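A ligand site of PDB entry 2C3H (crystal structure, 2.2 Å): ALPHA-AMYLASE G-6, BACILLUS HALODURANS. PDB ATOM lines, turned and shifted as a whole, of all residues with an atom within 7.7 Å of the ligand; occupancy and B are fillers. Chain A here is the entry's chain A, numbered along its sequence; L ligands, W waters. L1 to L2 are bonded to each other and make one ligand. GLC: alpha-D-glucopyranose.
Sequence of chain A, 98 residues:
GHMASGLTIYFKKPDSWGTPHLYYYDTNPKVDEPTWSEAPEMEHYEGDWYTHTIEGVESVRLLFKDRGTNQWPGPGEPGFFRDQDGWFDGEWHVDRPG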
ATOM      1  N   TYR A  23      12.194  15.665  18.951  1.00  0.00           N
ATOM      2  CA  TYR A  23      11.957  14.693  17.887  1.00  0.00           C
ATOM      3  C   TYR A  23      10.671  13.962  18.227  1.00  0.00           C
ATOM      4  O   TYR A  23      10.423  13.657  19.423  1.00  0.00           O
ATOM      5  CB  TYR A  23      13.165  13.754  17.694  1.00  0.00           C
ATOM      6  CG  TYR A  23      12.851  12.603  16.784  1.00  0.00           C
ATOM      7  CD1 TYR A  23      12.931  12.754  15.385  1.00  0.00           C
ATOM      8  CD2 TYR A  23      12.434  11.377  17.297  1.00  0.00           C
ATOM      9  CE1 TYR A  23      12.628  11.706  14.530  1.00  0.00           C
ATOM     10  CE2 TYR A  23      12.121  10.320  16.448  1.00  0.00           C
ATOM     11  CZ  TYR A  23      12.215  10.515  15.054  1.00  0.00           C
ATOM     12  OH  TYR A  23      11.901   9.517  14.171  1.00  0.00           O
ATOM     13  N   TYR A  24       9.819  13.684  17.224  1.00  0.00           N
ATOM     14  CA  TYR A  24       8.541  13.032  17.509  1.00  0.00           C
ATOM     15  C   TYR A  24       8.041  12.175  16.351  1.00  0.00           C
ATOM     16  O   TYR A  24       8.319  12.476  15.212  1.00  0.00           O
ATOM     17  CB  TYR A  24       7.488  14.076  17.907  1.00  0.00           C
ATOM     18  CG  TYR A  24       7.255  15.207  16.899  1.00  0.00           C
ATOM     19  CD1 TYR A  24       7.995  16.409  16.980  1.00  0.00           C
ATOM     20  CD2 TYR A  24       6.281  15.067  15.896  1.00  0.00           C
ATOM     21  CE1 TYR A  24       7.774  17.422  16.087  1.00  0.00           C
ATOM     22  CE2 TYR A  24       6.060  16.072  14.975  1.00  0.00           C
ATOM     23  CZ  TYR A  24       6.804  17.232  15.064  1.00  0.00           C
ATOM     24  OH  TYR A  24       6.560  18.246  14.171  1.00  0.00           O
ATOM     25  N   TYR A  25       7.316  11.105  16.642  1.00  0.00           N
ATOM     26  CA  TYR A  25       6.795  10.225  15.587  1.00  0.00           C
ATOM     27  C   TYR A  25       5.554   9.611  16.184  1.00  0.00           C
ATOM     28  O   TYR A  25       5.182   9.978  17.320  1.00  0.00           O
ATOM     29  CB  TYR A  25       7.840   9.177  15.186  1.00  0.00           C
ATOM     30  CG  TYR A  25       8.244   8.251  16.322  1.00  0.00           C
ATOM     31  CD1 TYR A  25       9.150   8.687  17.310  1.00  0.00           C
ATOM     32  CD2 TYR A  25       7.720   6.958  16.418  1.00  0.00           C
ATOM     33  CE1 TYR A  25       9.541   7.827  18.368  1.00  0.00           C
ATOM     34  CE2 TYR A  25       8.101   6.084  17.491  1.00  0.00           C
ATOM     35  CZ  TYR A  25       9.027   6.554  18.442  1.00  0.00           C
ATOM     36  OH  TYR A  25       9.406   5.776  19.505  1.00  0.00           O
ATOM     37  N   ASP A  26       4.911   8.694  15.434  1.00  0.00           N
ATOM     38  CA  ASP A  26       3.608   8.156  15.766  1.00  0.00           C
ATOM     39  C   ASP A  26       2.594   9.260  16.063  1.00  0.00           C
ATOM     40  O   ASP A  26       1.803   9.112  17.003  1.00  0.00           O
ATOM     41  CB  ASP A  26       3.675   7.283  17.029  1.00  0.00           C
ATOM     42  CG  ASP A  26       4.161   5.890  16.749  1.00  0.00           C
ATOM     43  OD1 ASP A  26       4.736   5.634  15.645  1.00  0.00           O
ATOM     44  OD2 ASP A  26       4.032   4.973  17.605  1.00  0.00           O
ATOM     45  N   GLU A  33       6.352  14.618   9.969  1.00  0.00           N
ATOM     46  CA  GLU A  33       7.277  14.114  10.972  1.00  0.00           C
ATOM     47  C   GLU A  33       8.744  14.328  10.556  1.00  0.00           C
ATOM     48  O   GLU A  33       9.241  13.677   9.636  1.00  0.00           O
ATOM     49  CB  GLU A  33       7.003  12.636  11.222  1.00  0.00           C
ATOM     50  CG  GLU A  33       5.837  12.378  12.182  1.00  0.00           C
ATOM     51  CD  GLU A  33       5.347  10.939  12.209  1.00  0.00           C
ATOM     52  OE1 GLU A  33       6.074  10.025  11.760  1.00  0.00           O
ATOM     53  OE2 GLU A  33       4.235  10.683  12.685  1.00  0.00           O
ATOM     54  N   PRO A  34       9.436  15.270  11.182  1.00  0.00           N
ATOM     55  CA  PRO A  34      10.867  15.448  10.897  1.00  0.00           C
ATOM     56  C   PRO A  34      11.710  14.236  11.166  1.00  0.00           C
ATOM     57  O   PRO A  34      11.468  13.464  12.063  1.00  0.00           O
ATOM     58  CB  PRO A  34      11.307  16.536  11.879  1.00  0.00           C
ATOM     59  CG  PRO A  34      10.290  16.555  12.869  1.00  0.00           C
ATOM     60  CD  PRO A  34       8.957  16.279  12.132  1.00  0.00           C
ATOM     61  N   THR A  35      12.684  14.092  10.296  1.00  0.00           N
ATOM     62  CA  THR A  35      13.926  13.392  10.533  1.00  0.00           C
ATOM     63  C   THR A  35      14.640  13.757  11.882  1.00  0.00           C
ATOM     64  O   THR A  35      14.544  14.864  12.353  1.00  0.00           O
ATOM     65  CB  THR A  35      14.776  13.814   9.331  1.00  0.00           C
ATOM     66  OG1 THR A  35      14.553  12.857   8.276  1.00  0.00           O
ATOM     67  CG2 THR A  35      16.208  13.742   9.599  1.00  0.00           C
ATOM     68  N   TRP A  36      15.314  12.778  12.485  1.00  0.00           N
ATOM     69  CA  TRP A  36      16.171  12.963  13.666  1.00  0.00           C
ATOM     70  C   TRP A  36      16.982  14.280  13.586  1.00  0.00           C
ATOM     71  O   TRP A  36      16.902  15.120  14.504  1.00  0.00           O
ATOM     72  CB  TRP A  36      17.115  11.745  13.828  1.00  0.00           C
ATOM     73  CG  TRP A  36      17.929  11.743  15.101  1.00  0.00           C
ATOM     74  CD1 TRP A  36      19.282  11.921  15.229  1.00  0.00           C
ATOM     75  CD2 TRP A  36      17.421  11.547  16.428  1.00  0.00           C
ATOM     76  NE1 TRP A  36      19.645  11.839  16.550  1.00  0.00           N
ATOM     77  CE2 TRP A  36      18.513  11.625  17.301  1.00  0.00           C
ATOM     78  CE3 TRP A  36      16.142  11.302  16.963  1.00  0.00           C
ATOM     79  CZ2 TRP A  36      18.355  11.502  18.667  1.00  0.00           C
ATOM     80  CZ3 TRP A  36      15.999  11.173  18.289  1.00  0.00           C
ATOM     81  CH2 TRP A  36      17.087  11.251  19.138  1.00  0.00           C
ATOM     82  N   SER A  37      17.726  14.479  12.474  1.00  0.00           N
ATOM     83  CA  SER A  37      18.632  15.638  12.357  1.00  0.00           C
ATOM     84  C   SER A  37      17.881  16.932  12.084  1.00  0.00           C
ATOM     85  O   SER A  37      18.406  18.022  12.251  1.00  0.00           O
ATOM     86  CB  SER A  37      19.704  15.447  11.294  1.00  0.00           C
ATOM     87  OG  SER A  37      19.121  15.111  10.064  1.00  0.00           O
ATOM     88  N   ARG A  61       4.688  10.115  20.218  1.00  0.00           N
ATOM     89  CA  ARG A  61       5.890   9.600  20.904  1.00  0.00           C
ATOM     90  C   ARG A  61       7.029  10.571  20.629  1.00  0.00           C
ATOM     91  O   ARG A  61       7.230  11.063  19.491  1.00  0.00           O
ATOM     92  CB  ARG A  61       6.247   8.187  20.451  1.00  0.00           C
ATOM     93  CG  ARG A  61       5.226   7.156  20.932  1.00  0.00           C
ATOM     94  CD  ARG A  61       5.633   5.694  20.711  1.00  0.00           C
ATOM     95  NE  ARG A  61       4.734   4.825  21.468  1.00  0.00           N
ATOM     96  CZ  ARG A  61       3.537   4.412  21.017  1.00  0.00           C
ATOM     97  NH1 ARG A  61       2.797   3.628  21.765  1.00  0.00           N
ATOM     98  NH2 ARG A  61       3.088   4.773  19.802  1.00  0.00           N
ATOM     99  N   LEU A  62       7.768  10.898  21.682  1.00  0.00           N
ATOM    100  CA  LEU A  62       8.770  11.924  21.531  1.00  0.00           C
ATOM    101  C   LEU A  62      10.099  11.625  22.219  1.00  0.00           C
ATOM    102  O   LEU A  62      10.160  10.945  23.248  1.00  0.00           O
ATOM    103  CB  LEU A  62       8.200  13.306  21.919  1.00  0.00           C
ATOM    104  CG  LEU A  62       7.868  13.508  23.402  1.00  0.00           C
ATOM    105  CD1 LEU A  62       9.037  14.025  24.335  1.00  0.00           C
ATOM    106  CD2 LEU A  62       6.663  14.409  23.488  1.00  0.00           C
ATOM    107  N   LEU A  63      11.172  12.163  21.650  1.00  0.00           N
ATOM    108  CA  LEU A  63      12.468  12.113  22.307  1.00  0.00           C
ATOM    109  C   LEU A  63      13.028  13.530  22.339  1.00  0.00           C
ATOM    110  O   LEU A  63      12.833  14.296  21.383  1.00  0.00           O
ATOM    111  CB  LEU A  63      13.410  11.201  21.548  1.00  0.00           C
ATOM    112  CG  LEU A  63      13.127   9.717  21.650  1.00  0.00           C
ATOM    113  CD1 LEU A  63      12.105   9.294  20.511  1.00  0.00           C
ATOM    114  CD2 LEU A  63      14.390   8.893  21.641  1.00  0.00           C
ATOM    115  N   LYS A  65      16.536  15.720  22.158  1.00  0.00           N
ATOM    116  CA  LYS A  65      17.927  15.680  21.658  1.00  0.00           C
ATOM    117  C   LYS A  65      18.530  17.103  21.614  1.00  0.00           C
ATOM    118  O   LYS A  65      17.804  18.114  21.780  1.00  0.00           O
ATOM    119  CB  LYS A  65      18.028  15.062  20.230  1.00  0.00           C
ATOM    120  CG  LYS A  65      17.019  15.614  19.219  1.00  0.00           C
ATOM    121  CD  LYS A  65      17.125  14.919  17.836  1.00  0.00           C
ATOM    122  CE  LYS A  65      18.612  14.777  17.336  1.00  0.00           C
ATOM    123  NZ  LYS A  65      19.268  16.109  17.044  1.00  0.00           N
ATOM    124  N   THR A  69      25.090  14.621  19.978  1.00  0.00           N
ATOM    125  CA  THR A  69      24.696  13.220  20.117  1.00  0.00           C
ATOM    126  C   THR A  69      23.888  12.934  21.373  1.00  0.00           C
ATOM    127  O   THR A  69      23.660  11.755  21.710  1.00  0.00           O
ATOM    128  CB  THR A  69      25.942  12.290  20.158  1.00  0.00           C
ATOM    129  OG1 THR A  69      26.717  12.591  21.350  1.00  0.00           O
ATOM    130  CG2 THR A  69      26.865  12.595  18.980  1.00  0.00           C
ATOM    131  N   ASN A  70      23.482  13.955  22.096  1.00  0.00           N
ATOM    132  CA  ASN A  70      22.761  13.696  23.324  1.00  0.00           C
ATOM    133  C   ASN A  70      21.314  13.434  22.948  1.00  0.00           C
ATOM    134  O   ASN A  70      20.779  13.994  21.987  1.00  0.00           O
ATOM    135  CB  ASN A  70      22.832  14.897  24.267  1.00  0.00           C
ATOM    136  CG  ASN A  70      24.249  15.199  24.764  1.00  0.00           C
ATOM    137  OD1 ASN A  70      24.734  16.359  24.675  1.00  0.00           O
ATOM    138  ND2 ASN A  70      24.929  14.184  25.283  1.00  0.00           N
ATOM    139  N   GLN A  71      20.670  12.581  23.727  1.00  0.00           N
ATOM    140  CA  GLN A  71      19.229  12.373  23.563  1.00  0.00           C
ATOM    141  C   GLN A  71      18.738  11.784  24.864  1.00  0.00           C
ATOM    142  O   GLN A  71      19.498  11.213  25.650  1.00  0.00           O
ATOM    143  CB  GLN A  71      18.849  11.460  22.375  1.00  0.00           C
ATOM    144  CG  GLN A  71      19.459  10.065  22.469  1.00  0.00           C
ATOM    145  CD  GLN A  71      19.067   9.205  21.291  1.00  0.00           C
ATOM    146  OE1 GLN A  71      18.020   8.540  21.303  1.00  0.00           O
ATOM    147  NE2 GLN A  71      19.859   9.267  20.235  1.00  0.00           N
ATOM    148  N   PRO A  73      14.946   9.749  25.716  1.00  0.00           N
ATOM    149  CA  PRO A  73      15.768   8.594  26.128  1.00  0.00           C
ATOM    150  C   PRO A  73      16.837   8.147  25.115  1.00  0.00           C
ATOM    151  O   PRO A  73      16.973   8.741  24.027  1.00  0.00           O
ATOM    152  CB  PRO A  73      14.728   7.508  26.299  1.00  0.00           C
ATOM    153  CG  PRO A  73      13.807   7.779  25.254  1.00  0.00           C
ATOM    154  CD  PRO A  73      13.617   9.305  25.299  1.00  0.00           C
ATOM    155  N   GLY A  74      17.583   7.103  25.488  1.00  0.00           N
ATOM    156  CA  GLY A  74      18.709   6.584  24.753  1.00  0.00           C
ATOM    157  C   GLY A  74      18.467   6.205  23.296  1.00  0.00           C
ATOM    158  O   GLY A  74      17.345   6.057  22.805  1.00  0.00           O
ATOM    159  N   PRO A  75      19.565   5.998  22.581  1.00  0.00           N
ATOM    160  CA  PRO A  75      19.456   5.631  21.185  1.00  0.00           C
ATOM    161  C   PRO A  75      18.542   4.428  21.048  1.00  0.00           C
ATOM    162  O   PRO A  75      18.738   3.410  21.735  1.00  0.00           O
ATOM    163  CB  PRO A  75      20.912   5.296  20.821  1.00  0.00           C
ATOM    164  CG  PRO A  75      21.691   6.115  21.728  1.00  0.00           C
ATOM    165  CD  PRO A  75      20.973   6.100  23.031  1.00  0.00           C
ATOM    166  N   GLY A  76      17.518   4.555  20.203  1.00  0.00           N
ATOM    167  CA  GLY A  76      16.674   3.410  19.869  1.00  0.00           C
ATOM    168  C   GLY A  76      15.526   3.173  20.854  1.00  0.00           C
ATOM    169  O   GLY A  76      14.580   2.459  20.554  1.00  0.00           O
ATOM    170  N   GLU A  77      15.606   3.765  22.048  1.00  0.00           N
ATOM    171  CA  GLU A  77      14.533   3.529  23.038  1.00  0.00           C
ATOM    172  C   GLU A  77      13.272   4.224  22.536  1.00  0.00           C
ATOM    173  O   GLU A  77      13.335   5.336  21.982  1.00  0.00           O
ATOM    174  CB  GLU A  77      14.916   4.091  24.417  1.00  0.00           C
ATOM    175  CG  GLU A  77      16.163   3.480  25.044  1.00  0.00           C
ATOM    176  CD  GLU A  77      15.964   2.022  25.501  1.00  0.00           C
ATOM    177  OE1 GLU A  77      16.961   1.388  25.911  1.00  0.00           O
ATOM    178  OE2 GLU A  77      14.828   1.464  25.448  1.00  0.00           O
ATOM    179  N   PRO A  78      12.114   3.648  22.768  1.00  0.00           N
ATOM    180  CA  PRO A  78      10.872   4.299  22.334  1.00  0.00           C
ATOM    181  C   PRO A  78      10.710   5.709  22.889  1.00  0.00           C
ATOM    182  O   PRO A  78      11.138   6.025  24.028  1.00  0.00           O
ATOM    183  CB  PRO A  78       9.728   3.394  22.878  1.00  0.00           C
ATOM    184  CG  PRO A  78      10.424   2.141  23.543  1.00  0.00           C
ATOM    185  CD  PRO A  78      11.904   2.379  23.501  1.00  0.00           C
ATOM    186  N   GLY A  79      10.078   6.555  22.096  1.00  0.00           N
ATOM    187  CA  GLY A  79       9.721   7.900  22.530  1.00  0.00           C
ATOM    188  C   GLY A  79       8.874   7.868  23.804  1.00  0.00           C
ATOM    189  O   GLY A  79       8.256   6.822  24.114  1.00  0.00           O
HETATM  190  C1  GLC L   1      18.578   7.932  16.046  1.00  0.00           C
HETATM  191  C2  GLC L   1      18.213   7.903  17.533  1.00  0.00           C
HETATM  192  C3  GLC L   1      17.028   6.978  17.754  1.00  0.00           C
HETATM  193  C4  GLC L   1      15.875   7.473  16.890  1.00  0.00           C
HETATM  194  C5  GLC L   1      16.288   7.497  15.436  1.00  0.00           C
HETATM  195  C6  GLC L   1      15.148   8.013  14.575  1.00  0.00           C
HETATM  196  O1  GLC L   1      19.080   6.678  15.642  1.00  0.00           O
HETATM  197  O2  GLC L   1      19.303   7.487  18.315  1.00  0.00           O
HETATM  198  O3  GLC L   1      16.584   6.879  19.110  1.00  0.00           O
HETATM  199  O4  GLC L   1      14.851   6.534  17.073  1.00  0.00           O
HETATM  200  O5  GLC L   1      17.455   8.302  15.246  1.00  0.00           O
HETATM  201  O6  GLC L   1      15.465   8.003  13.190  1.00  0.00           O
HETATM  202  C1  GLC L   2      13.388   6.815  17.795  1.00  0.00           C
HETATM  203  C2  GLC L   2      13.090   5.779  18.852  1.00  0.00           C
HETATM  204  C3  GLC L   2      12.863   4.432  18.213  1.00  0.00           C
HETATM  205  C4  GLC L   2      11.805   4.559  17.104  1.00  0.00           C
HETATM  206  C5  GLC L   2      12.259   5.555  16.064  1.00  0.00           C
HETATM  207  C6  GLC L   2      11.161   5.796  15.051  1.00  0.00           C
HETATM  208  O2  GLC L   2      14.214   5.670  19.677  1.00  0.00           O
HETATM  209  O3  GLC L   2      12.488   3.545  19.256  1.00  0.00           O
HETATM  210  O4  GLC L   2      11.562   3.326  16.478  1.00  0.00           O
HETATM  211  O5  GLC L   2      12.543   6.811  16.671  1.00  0.00           O
HETATM  212  O6  GLC L   2      11.486   6.911  14.248  1.00  0.00           O
HETATM  213  O   HOH W   1      19.805   6.452  13.208  1.00  0.00           O
HETATM  214  O   HOH W   2      21.826   6.272  17.254  1.00  0.00           O
HETATM  215  O   HOH W   3      15.082   9.974  10.978  1.00  0.00           O
HETATM  216  O   HOH W   4      14.779   5.776  12.297  1.00  0.00           O
HETATM  217  O   HOH W   5      19.090   8.885  12.397  1.00  0.00           O
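Water W3 bridges O6 of GLC L1 (3.0 Å) and N of Trp 36 (3.2 Å).
Merely in contact with the ligand: Tyr 25 (3.6 Å), Trp 36 (3.5 Å), Leu 63 (3.8 Å), Gly 74 (3.9 Å), Pro 75 (3.4 Å) and Pro 78 (3.5 Å). Within 4 Å of the ligand: Tyr 23, Tyr 25, Trp 36, Leu 63, Gln 71, Gly 74, Pro 75, Gly 76, Glu 77 and Pro 78.
The backbone carbonyl oxygen (O) of Gly 76 is in hydrogen-bond range of an oxygen (O3) of GLC L2 (2.7 Å). O2 of GLC L2 lies within hydrogen-bond range of O of Glu 77 (2.5 Å). The backbone NH of Glu 77 lies close to an oxygen (O2) of GLC L2, at 3.3 Å. An oxygen (O2) of GLC L1 sits at hydrogen-bond distance from the side-chain amide nitrogen (NE2) of Gln 71 (2.7 Å). The backbone NH (N) of Gly 76 is in hydrogen-bond range of an oxygen (O3) of GLC L1 (2.7 Å). The side-chain hydroxyl (OH) of Tyr 23 lies within hydrogen-bond range of an oxygen (O6) of GLC L2.
OE1 of Gln 71 sits close to O of Pro 73, at 2.9 Å. N of Tyr 25 lies within hydrogen-bond range of O of Arg 61, at 2.9 Å. The side-chain amide oxygen of Gln 71 lies close to the backbone carbonyl oxygen of Gly 74 (3.0 Å). N of Gly 79 lies within hydrogen-bond range of OH of Tyr 25 (2.8 Å). O of Tyr 23 sits at hydrogen-bond distance from N of Leu 63 (2.8 Å).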
